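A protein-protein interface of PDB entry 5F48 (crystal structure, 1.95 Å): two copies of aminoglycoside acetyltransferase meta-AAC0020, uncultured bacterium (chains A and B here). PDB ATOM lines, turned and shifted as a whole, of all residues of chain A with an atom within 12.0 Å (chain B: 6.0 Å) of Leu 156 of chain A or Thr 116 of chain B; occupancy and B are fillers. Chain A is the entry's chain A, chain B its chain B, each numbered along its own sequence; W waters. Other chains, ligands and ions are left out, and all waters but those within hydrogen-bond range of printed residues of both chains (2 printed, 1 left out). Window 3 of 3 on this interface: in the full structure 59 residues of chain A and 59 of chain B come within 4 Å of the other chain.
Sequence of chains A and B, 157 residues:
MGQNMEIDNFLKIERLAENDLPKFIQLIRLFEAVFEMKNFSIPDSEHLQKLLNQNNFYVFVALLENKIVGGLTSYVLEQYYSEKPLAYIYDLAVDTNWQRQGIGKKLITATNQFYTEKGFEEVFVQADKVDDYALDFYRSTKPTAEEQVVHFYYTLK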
ATOM      1  N   PHE A 152       8.347 -32.765   4.109  1.00  0.00           N
ATOM      2  CA  PHE A 152       7.678 -31.577   3.587  1.00  0.00           C
ATOM      3  C   PHE A 152       7.838 -31.516   2.083  1.00  0.00           C
ATOM      4  O   PHE A 152       8.932 -31.767   1.571  1.00  0.00           O
ATOM      5  CB  PHE A 152       8.258 -30.306   4.174  1.00  0.00           C
ATOM      6  CG  PHE A 152       8.155 -30.213   5.668  1.00  0.00           C
ATOM      7  CD1 PHE A 152       7.059 -29.610   6.262  1.00  0.00           C
ATOM      8  CD2 PHE A 152       9.167 -30.702   6.467  1.00  0.00           C
ATOM      9  CE1 PHE A 152       6.966 -29.499   7.633  1.00  0.00           C
ATOM     10  CE2 PHE A 152       9.074 -30.608   7.846  1.00  0.00           C
ATOM     11  CZ  PHE A 152       7.974 -29.995   8.419  1.00  0.00           C
ATOM     12  N   TYR A 153       6.786 -31.143   1.372  1.00  0.00           N
ATOM     13  CA  TYR A 153       6.983 -30.906  -0.052  1.00  0.00           C
ATOM     14  C   TYR A 153       6.341 -29.617  -0.558  1.00  0.00           C
ATOM     15  O   TYR A 153       5.368 -29.104   0.004  1.00  0.00           O
ATOM     16  CB  TYR A 153       6.501 -32.115  -0.875  1.00  0.00           C
ATOM     17  CG  TYR A 153       5.005 -32.383  -0.900  1.00  0.00           C
ATOM     18  CD1 TYR A 153       4.168 -31.705  -1.779  1.00  0.00           C
ATOM     19  CD2 TYR A 153       4.440 -33.367  -0.086  1.00  0.00           C
ATOM     20  CE1 TYR A 153       2.802 -31.971  -1.815  1.00  0.00           C
ATOM     21  CE2 TYR A 153       3.065 -33.645  -0.124  1.00  0.00           C
ATOM     22  CZ  TYR A 153       2.261 -32.948  -0.986  1.00  0.00           C
ATOM     23  OH  TYR A 153       0.913 -33.212  -1.026  1.00  0.00           O
ATOM     24  N   TYR A 154       6.949 -29.095  -1.622  1.00  0.00           N
ATOM     25  CA  TYR A 154       6.478 -27.899  -2.299  1.00  0.00           C
ATOM     26  C   TYR A 154       6.077 -28.279  -3.722  1.00  0.00           C
ATOM     27  O   TYR A 154       6.939 -28.620  -4.535  1.00  0.00           O
ATOM     28  CB  TYR A 154       7.560 -26.822  -2.337  1.00  0.00           C
ATOM     29  CG  TYR A 154       8.261 -26.585  -1.017  1.00  0.00           C
ATOM     30  CD1 TYR A 154       9.267 -27.429  -0.583  1.00  0.00           C
ATOM     31  CD2 TYR A 154       7.924 -25.507  -0.216  1.00  0.00           C
ATOM     32  CE1 TYR A 154       9.904 -27.222   0.609  1.00  0.00           C
ATOM     33  CE2 TYR A 154       8.558 -25.295   0.982  1.00  0.00           C
ATOM     34  CZ  TYR A 154       9.546 -26.150   1.383  1.00  0.00           C
ATOM     35  OH  TYR A 154      10.187 -25.928   2.563  1.00  0.00           O
ATOM     36  N   THR A 155       4.782 -28.239  -4.009  1.00  0.00           N
ATOM     37  CA  THR A 155       4.298 -28.468  -5.368  1.00  0.00           C
ATOM     38  C   THR A 155       4.547 -27.229  -6.219  1.00  0.00           C
ATOM     39  O   THR A 155       4.051 -26.151  -5.908  1.00  0.00           O
ATOM     40  CB  THR A 155       2.810 -28.831  -5.363  1.00  0.00           C
ATOM     41  OG1 THR A 155       2.621 -29.984  -4.528  1.00  0.00           O
ATOM     42  CG2 THR A 155       2.323 -29.137  -6.759  1.00  0.00           C
ATOM     43  N   LEU A 156       5.311 -27.374  -7.298  1.00  0.00           N
ATOM     44  CA  LEU A 156       5.736 -26.201  -8.052  1.00  0.00           C
ATOM     45  C   LEU A 156       4.726 -25.813  -9.131  1.00  0.00           C
ATOM     46  O   LEU A 156       3.944 -26.650  -9.594  1.00  0.00           O
ATOM     47  CB  LEU A 156       7.114 -26.440  -8.678  1.00  0.00           C
ATOM     48  CG  LEU A 156       8.243 -26.932  -7.761  1.00  0.00           C
ATOM     49  CD1 LEU A 156       9.581 -27.004  -8.519  1.00  0.00           C
ATOM     50  CD2 LEU A 156       8.381 -26.072  -6.496  1.00  0.00           C
ATOM     51  N   LYS A 157       4.751 -24.542  -9.524  1.00  0.00           N
ATOM     52  CA  LYS A 157       3.928 -24.056 -10.627  1.00  0.00           C
ATOM     53  C   LYS A 157       4.583 -24.395 -11.962  1.00  0.00           C
ATOM     54  O   LYS A 157       3.995 -24.230 -13.035  1.00  0.00           O
ATOM     55  CB  LYS A 157       3.709 -22.547 -10.529  1.00  0.00           C
ATOM     56  CG  LYS A 157       3.298 -22.059  -9.152  1.00  0.00           C
ATOM     57  CD  LYS A 157       2.050 -22.752  -8.656  1.00  0.00           C
ATOM     58  CE  LYS A 157       1.377 -21.916  -7.579  1.00  0.00           C
ATOM     59  NZ  LYS A 157       0.880 -20.610  -8.125  1.00  0.00           N
ATOM     60  OXT LYS A 157       5.729 -24.842 -11.995  1.00  0.00           O
ATOM     61  N   THR B 111      15.759 -21.932  -4.012  1.00  0.00           N
ATOM     62  CA  THR B 111      15.852 -23.310  -4.477  1.00  0.00           C
ATOM     63  C   THR B 111      14.590 -23.694  -5.224  1.00  0.00           C
ATOM     64  O   THR B 111      14.646 -24.257  -6.326  1.00  0.00           O
ATOM     65  CB  THR B 111      16.102 -24.260  -3.310  1.00  0.00           C
ATOM     66  OG1 THR B 111      17.369 -23.924  -2.730  1.00  0.00           O
ATOM     67  CG2 THR B 111      16.125 -25.722  -3.786  1.00  0.00           C
ATOM     68  N   ASN B 112      13.446 -23.345  -4.659  1.00  0.00           N
ATOM     69  CA  ASN B 112      12.193 -23.659  -5.325  1.00  0.00           C
ATOM     70  C   ASN B 112      11.988 -22.839  -6.594  1.00  0.00           C
ATOM     71  O   ASN B 112      11.428 -23.326  -7.581  1.00  0.00           O
ATOM     72  CB  ASN B 112      11.044 -23.474  -4.340  1.00  0.00           C
ATOM     73  CG  ASN B 112      11.116 -24.487  -3.214  1.00  0.00           C
ATOM     74  OD1 ASN B 112      11.835 -25.490  -3.332  1.00  0.00           O
ATOM     75  ND2 ASN B 112      10.396 -24.240  -2.123  1.00  0.00           N
ATOM     76  N   GLN B 113      12.460 -21.601  -6.599  1.00  0.00           N
ATOM     77  CA  GLN B 113      12.327 -20.811  -7.814  1.00  0.00           C
ATOM     78  C   GLN B 113      13.126 -21.469  -8.942  1.00  0.00           C
ATOM     79  O   GLN B 113      12.632 -21.607 -10.056  1.00  0.00           O
ATOM     80  CB  GLN B 113      12.781 -19.367  -7.610  1.00  0.00           C
ATOM     81  CG  GLN B 113      12.559 -18.516  -8.848  1.00  0.00           C
ATOM     82  CD  GLN B 113      11.139 -18.664  -9.414  1.00  0.00           C
ATOM     83  OE1 GLN B 113      10.148 -18.642  -8.668  1.00  0.00           O
ATOM     84  NE2 GLN B 113      11.038 -18.836 -10.732  1.00  0.00           N
ATOM     85  N   PHE B 114      14.352 -21.882  -8.637  1.00  0.00           N
ATOM     86  CA  PHE B 114      15.226 -22.532  -9.616  1.00  0.00           C
ATOM     87  C   PHE B 114      14.578 -23.770 -10.228  1.00  0.00           C
ATOM     88  O   PHE B 114      14.494 -23.903 -11.444  1.00  0.00           O
ATOM     89  CB  PHE B 114      16.570 -22.917  -8.974  1.00  0.00           C
ATOM     90  CG  PHE B 114      17.454 -23.738  -9.868  1.00  0.00           C
ATOM     91  CD1 PHE B 114      18.082 -23.158 -10.972  1.00  0.00           C
ATOM     92  CD2 PHE B 114      17.666 -25.082  -9.614  1.00  0.00           C
ATOM     93  CE1 PHE B 114      18.893 -23.914 -11.812  1.00  0.00           C
ATOM     94  CE2 PHE B 114      18.480 -25.840 -10.437  1.00  0.00           C
ATOM     95  CZ  PHE B 114      19.099 -25.260 -11.540  1.00  0.00           C
ATOM     96  N   TYR B 115      14.104 -24.671  -9.381  1.00  0.00           N
ATOM     97  CA  TYR B 115      13.511 -25.901  -9.883  1.00  0.00           C
ATOM     98  C   TYR B 115      12.166 -25.635 -10.555  1.00  0.00           C
ATOM     99  O   TYR B 115      11.729 -26.411 -11.399  1.00  0.00           O
ATOM    100  CB  TYR B 115      13.387 -26.921  -8.752  1.00  0.00           C
ATOM    101  CG  TYR B 115      14.725 -27.545  -8.372  1.00  0.00           C
ATOM    102  CD1 TYR B 115      15.473 -28.225  -9.313  1.00  0.00           C
ATOM    103  CD2 TYR B 115      15.233 -27.453  -7.079  1.00  0.00           C
ATOM    104  CE1 TYR B 115      16.679 -28.798  -8.991  1.00  0.00           C
ATOM    105  CE2 TYR B 115      16.464 -28.034  -6.743  1.00  0.00           C
ATOM    106  CZ  TYR B 115      17.178 -28.715  -7.701  1.00  0.00           C
ATOM    107  OH  TYR B 115      18.410 -29.328  -7.408  1.00  0.00           O
ATOM    108  N   THR B 116      11.533 -24.512 -10.225  1.00  0.00           N
ATOM    109  CA  THR B 116      10.313 -24.106 -10.910  1.00  0.00           C
ATOM    110  C   THR B 116      10.662 -23.668 -12.337  1.00  0.00           C
ATOM    111  O   THR B 116       9.981 -24.041 -13.296  1.00  0.00           O
ATOM    112  CB  THR B 116       9.574 -22.962 -10.168  1.00  0.00           C
ATOM    113  OG1 THR B 116       9.176 -23.415  -8.862  1.00  0.00           O
ATOM    114  CG2 THR B 116       8.335 -22.501 -10.958  1.00  0.00           C
ATOM    115  N   GLU B 117      11.740 -22.903 -12.479  1.00  0.00           N
ATOM    116  CA  GLU B 117      12.193 -22.489 -13.808  1.00  0.00           C
ATOM    117  C   GLU B 117      12.564 -23.724 -14.628  1.00  0.00           C
ATOM    118  O   GLU B 117      12.353 -23.760 -15.835  1.00  0.00           O
ATOM    119  CB  GLU B 117      13.384 -21.528 -13.718  1.00  0.00           C
ATOM    120  CG  GLU B 117      13.021 -20.099 -13.281  1.00  0.00           C
ATOM    121  CD  GLU B 117      14.213 -19.340 -12.704  1.00  0.00           C
ATOM    122  OE1 GLU B 117      15.343 -19.884 -12.731  1.00  0.00           O
ATOM    123  OE2 GLU B 117      14.020 -18.208 -12.196  1.00  0.00           O
ATOM    124  N   LYS B 118      13.094 -24.745 -13.961  1.00  0.00           N
ATOM    125  CA  LYS B 118      13.502 -25.957 -14.655  1.00  0.00           C
ATOM    126  C   LYS B 118      12.331 -26.881 -14.966  1.00  0.00           C
ATOM    127  O   LYS B 118      12.503 -27.886 -15.638  1.00  0.00           O
ATOM    128  CB  LYS B 118      14.539 -26.718 -13.844  1.00  0.00           C
ATOM    129  CG  LYS B 118      15.954 -26.243 -14.030  1.00  0.00           C
ATOM    130  CD  LYS B 118      16.890 -27.126 -13.224  1.00  0.00           C
ATOM    131  CE  LYS B 118      17.244 -28.419 -13.944  1.00  0.00           C
ATOM    132  NZ  LYS B 118      18.278 -28.184 -14.992  1.00  0.00           N
ATOM    133  N   GLY B 119      11.143 -26.546 -14.478  1.00  0.00           N
ATOM    134  CA  GLY B 119       9.955 -27.317 -14.796  1.00  0.00           C
ATOM    135  C   GLY B 119       9.789 -28.596 -13.987  1.00  0.00           C
ATOM    136  O   GLY B 119       9.121 -29.529 -14.425  1.00  0.00           O
ATOM    137  N   PHE B 120      10.377 -28.626 -12.796  1.00  0.00           N
ATOM    138  CA  PHE B 120      10.245 -29.760 -11.879  1.00  0.00           C
ATOM    139  C   PHE B 120       8.825 -29.861 -11.321  1.00  0.00           C
ATOM    140  O   PHE B 120       8.141 -28.852 -11.170  1.00  0.00           O
ATOM    141  CB  PHE B 120      11.243 -29.640 -10.721  1.00  0.00           C
ATOM    142  CG  PHE B 120      12.647 -30.075 -11.069  1.00  0.00           C
ATOM    143  CD1 PHE B 120      13.261 -29.653 -12.240  1.00  0.00           C
ATOM    144  CD2 PHE B 120      13.361 -30.894 -10.202  1.00  0.00           C
ATOM    145  CE1 PHE B 120      14.547 -30.057 -12.545  1.00  0.00           C
ATOM    146  CE2 PHE B 120      14.651 -31.301 -10.498  1.00  0.00           C
ATOM    147  CZ  PHE B 120      15.249 -30.883 -11.668  1.00  0.00           C
ATOM    148  N   GLU B 121       8.387 -31.073 -11.008  1.00  0.00           N
ATOM    149  CA  GLU B 121       7.071 -31.253 -10.418  1.00  0.00           C
ATOM    150  C   GLU B 121       7.007 -30.745  -8.971  1.00  0.00           C
ATOM    151  O   GLU B 121       6.014 -30.155  -8.556  1.00  0.00           O
ATOM    152  CB  GLU B 121       6.668 -32.724 -10.461  1.00  0.00           C
ATOM    153  CG  GLU B 121       5.325 -33.008  -9.850  1.00  0.00           C
ATOM    154  CD  GLU B 121       5.030 -34.491  -9.779  1.00  0.00           C
ATOM    155  OE1 GLU B 121       5.716 -35.274 -10.469  1.00  0.00           O
ATOM    156  OE2 GLU B 121       4.110 -34.870  -9.029  1.00  0.00           O
ATOM    157  N   GLU B 122       8.074 -30.977  -8.214  1.00  0.00           N
ATOM    158  CA  GLU B 122       8.010 -30.830  -6.769  1.00  0.00           C
ATOM    159  C   GLU B 122       9.393 -30.880  -6.136  1.00  0.00           C
ATOM    160  O   GLU B 122      10.307 -31.546  -6.645  1.00  0.00           O
ATOM    161  CB  GLU B 122       7.112 -31.927  -6.180  1.00  0.00           C
ATOM    162  CG  GLU B 122       7.365 -32.275  -4.708  1.00  0.00           C
ATOM    163  CD  GLU B 122       6.559 -33.477  -4.244  1.00  0.00           C
ATOM    164  OE1 GLU B 122       5.371 -33.582  -4.605  1.00  0.00           O
ATOM    165  OE2 GLU B 122       7.134 -34.339  -3.554  1.00  0.00           O
ATOM    166  N   VAL B 123       9.548 -30.167  -5.029  1.00  0.00           N
ATOM    167  CA  VAL B 123      10.761 -30.249  -4.223  1.00  0.00           C
ATOM    168  C   VAL B 123      10.361 -30.774  -2.845  1.00  0.00           C
ATOM    169  O   VAL B 123       9.329 -30.362  -2.313  1.00  0.00           O
ATOM    170  CB  VAL B 123      11.446 -28.876  -4.100  1.00  0.00           C
ATOM    171  CG1 VAL B 123      12.592 -28.894  -3.053  1.00  0.00           C
ATOM    172  CG2 VAL B 123      11.939 -28.397  -5.463  1.00  0.00           C
ATOM    173  N   THR B 144       3.623 -27.046   0.688  1.00  0.00           N
ATOM    174  CA  THR B 144       2.304 -27.466   0.223  1.00  0.00           C
ATOM    175  C   THR B 144       1.671 -28.407   1.225  1.00  0.00           C
ATOM    176  O   THR B 144       0.507 -28.267   1.583  1.00  0.00           O
ATOM    177  CB  THR B 144       2.378 -28.176  -1.143  1.00  0.00           C
ATOM    178  OG1 THR B 144       2.966 -27.298  -2.106  1.00  0.00           O
ATOM    179  CG2 THR B 144       0.979 -28.583  -1.612  1.00  0.00           C
HETATM  180  O   HOH W   1       6.725 -22.864  -7.993  1.00  0.00           O
HETATM  181  O   HOH W   2       4.059 -29.242 -10.016  1.00  0.00           O
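Among the printed residues, merely in contact across the chains: Tyr 153 of chain A with Glu 122 of chain B, Tyr 153 of chain A with Val 123 of chain B, Tyr 154 of chain A with Asn 112 of chain B, Tyr 154 of chain A with Glu 122 of chain B, Tyr 154 of chain A with Thr 144 of chain B, Thr 155 of chain A with Glu 121 of chain B, Leu 156 of chain A with Tyr 115 of chain B, Leu 156 of chain A with Thr 116 of chain B, Leu 156 of chain A with Phe 120 of chain B and Lys 157 of chain A with Thr 116 of chain B.
Hydrophobic or aromatic side chains of chain B within 4 Å of the printed part of chain A: Tyr 115 and Phe 120. Of the 6 printed residues of chain A, 5 touch a printed residue of chain B. Hydrophobic or aromatic side chains of chain A that line the printed part of chain B: Tyr 153, Tyr 154 and Leu 156. Among the printed residues, 14 pairs touch across the chains. Among the printed residues, no Asp or Glu carboxylate lies within 4 Å of a Lys or Arg side-chain nitrogen of the other chain.
N of Thr 144 of chain B lies within hydrogen-bond range of O of Tyr 153 of chain A (2.8 Å). N of Tyr 154 of chain A sits at hydrogen-bond distance from O of Val 123 of chain B. The backbone NH of Thr 155 of chain A sits at hydrogen-bond distance from the side-chain hydroxyl of Thr 144 of chain B. N of Leu 156 of chain A is in hydrogen-bond range of O of Glu 121 of chain B, at 3.1 Å.
O of Asn 112 of chain B is in hydrogen-bond range of OG1 of Thr 116 of chain B (2.6 Å). N of Phe 120 of chain B is in hydrogen-bond range of O of Tyr 115 of chain B.
Water W2 lies within hydrogen-bond range of O of Glu 121 of chain B and O of Leu 156 of chain A. Water W1 bridges the side-chain hydroxyl of Thr 116 of chain B (2.7 Å) and the backbone NH of Lys 157 of chain A (3.0 Å).
No position is printed for both chains. Of the 14 pairs that touch across the chains among the printed residues, none has its exchanged pair printed and touching as well.
Of the printed residues of chain B, Tyr 153 of chain A touches Glu 122 (3.5 Å), Val 123 (3.3 Å) and Thr 144 (2.8 Å). Of chain B, only Tyr 115 (3.6 Å), Thr 116 (3.6 Å), Phe 120 (3.5 Å) and Glu 121 (3.1 Å) come within 4 Å of Leu 156 of chain A. Of the printed residues of chain B, Lys 157 of chain A touches Thr 116 (3.7 Å). No residue of chain A comes within 4 Å of Phe 114 of chain B. Of the printed residues of chain A, Tyr 115 of chain B touches Leu 156 (3.6 Å). No residue of chain A comes within 4 Å of Glu 117 of chain B. Lys 118 of chain B touches none of the printed residues of chain A. No residue of chain A comes within 4 Å of Gly 119 of chain B. Of chain A, only Leu 156 (3.5 Å) comes within 4 Å of Phe 120 of chain B. Of the printed residues of chain A, Glu 121 of chain B touches Thr 155 and Leu 156. Of the printed residues of chain A, Glu 122 of chain B touches Tyr 153 (3.5 Å) and Tyr 154 (3.3 Å). Val 123 of chain B touches two residues of chain A. The nearest residue of chain B that does not touch Leu 156 of chain A is Glu 122 of chain B (4.03 Å). The nearest residue of chain A that does not touch Thr 116 of chain B is Thr 155 of chain A (6.5 Å).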
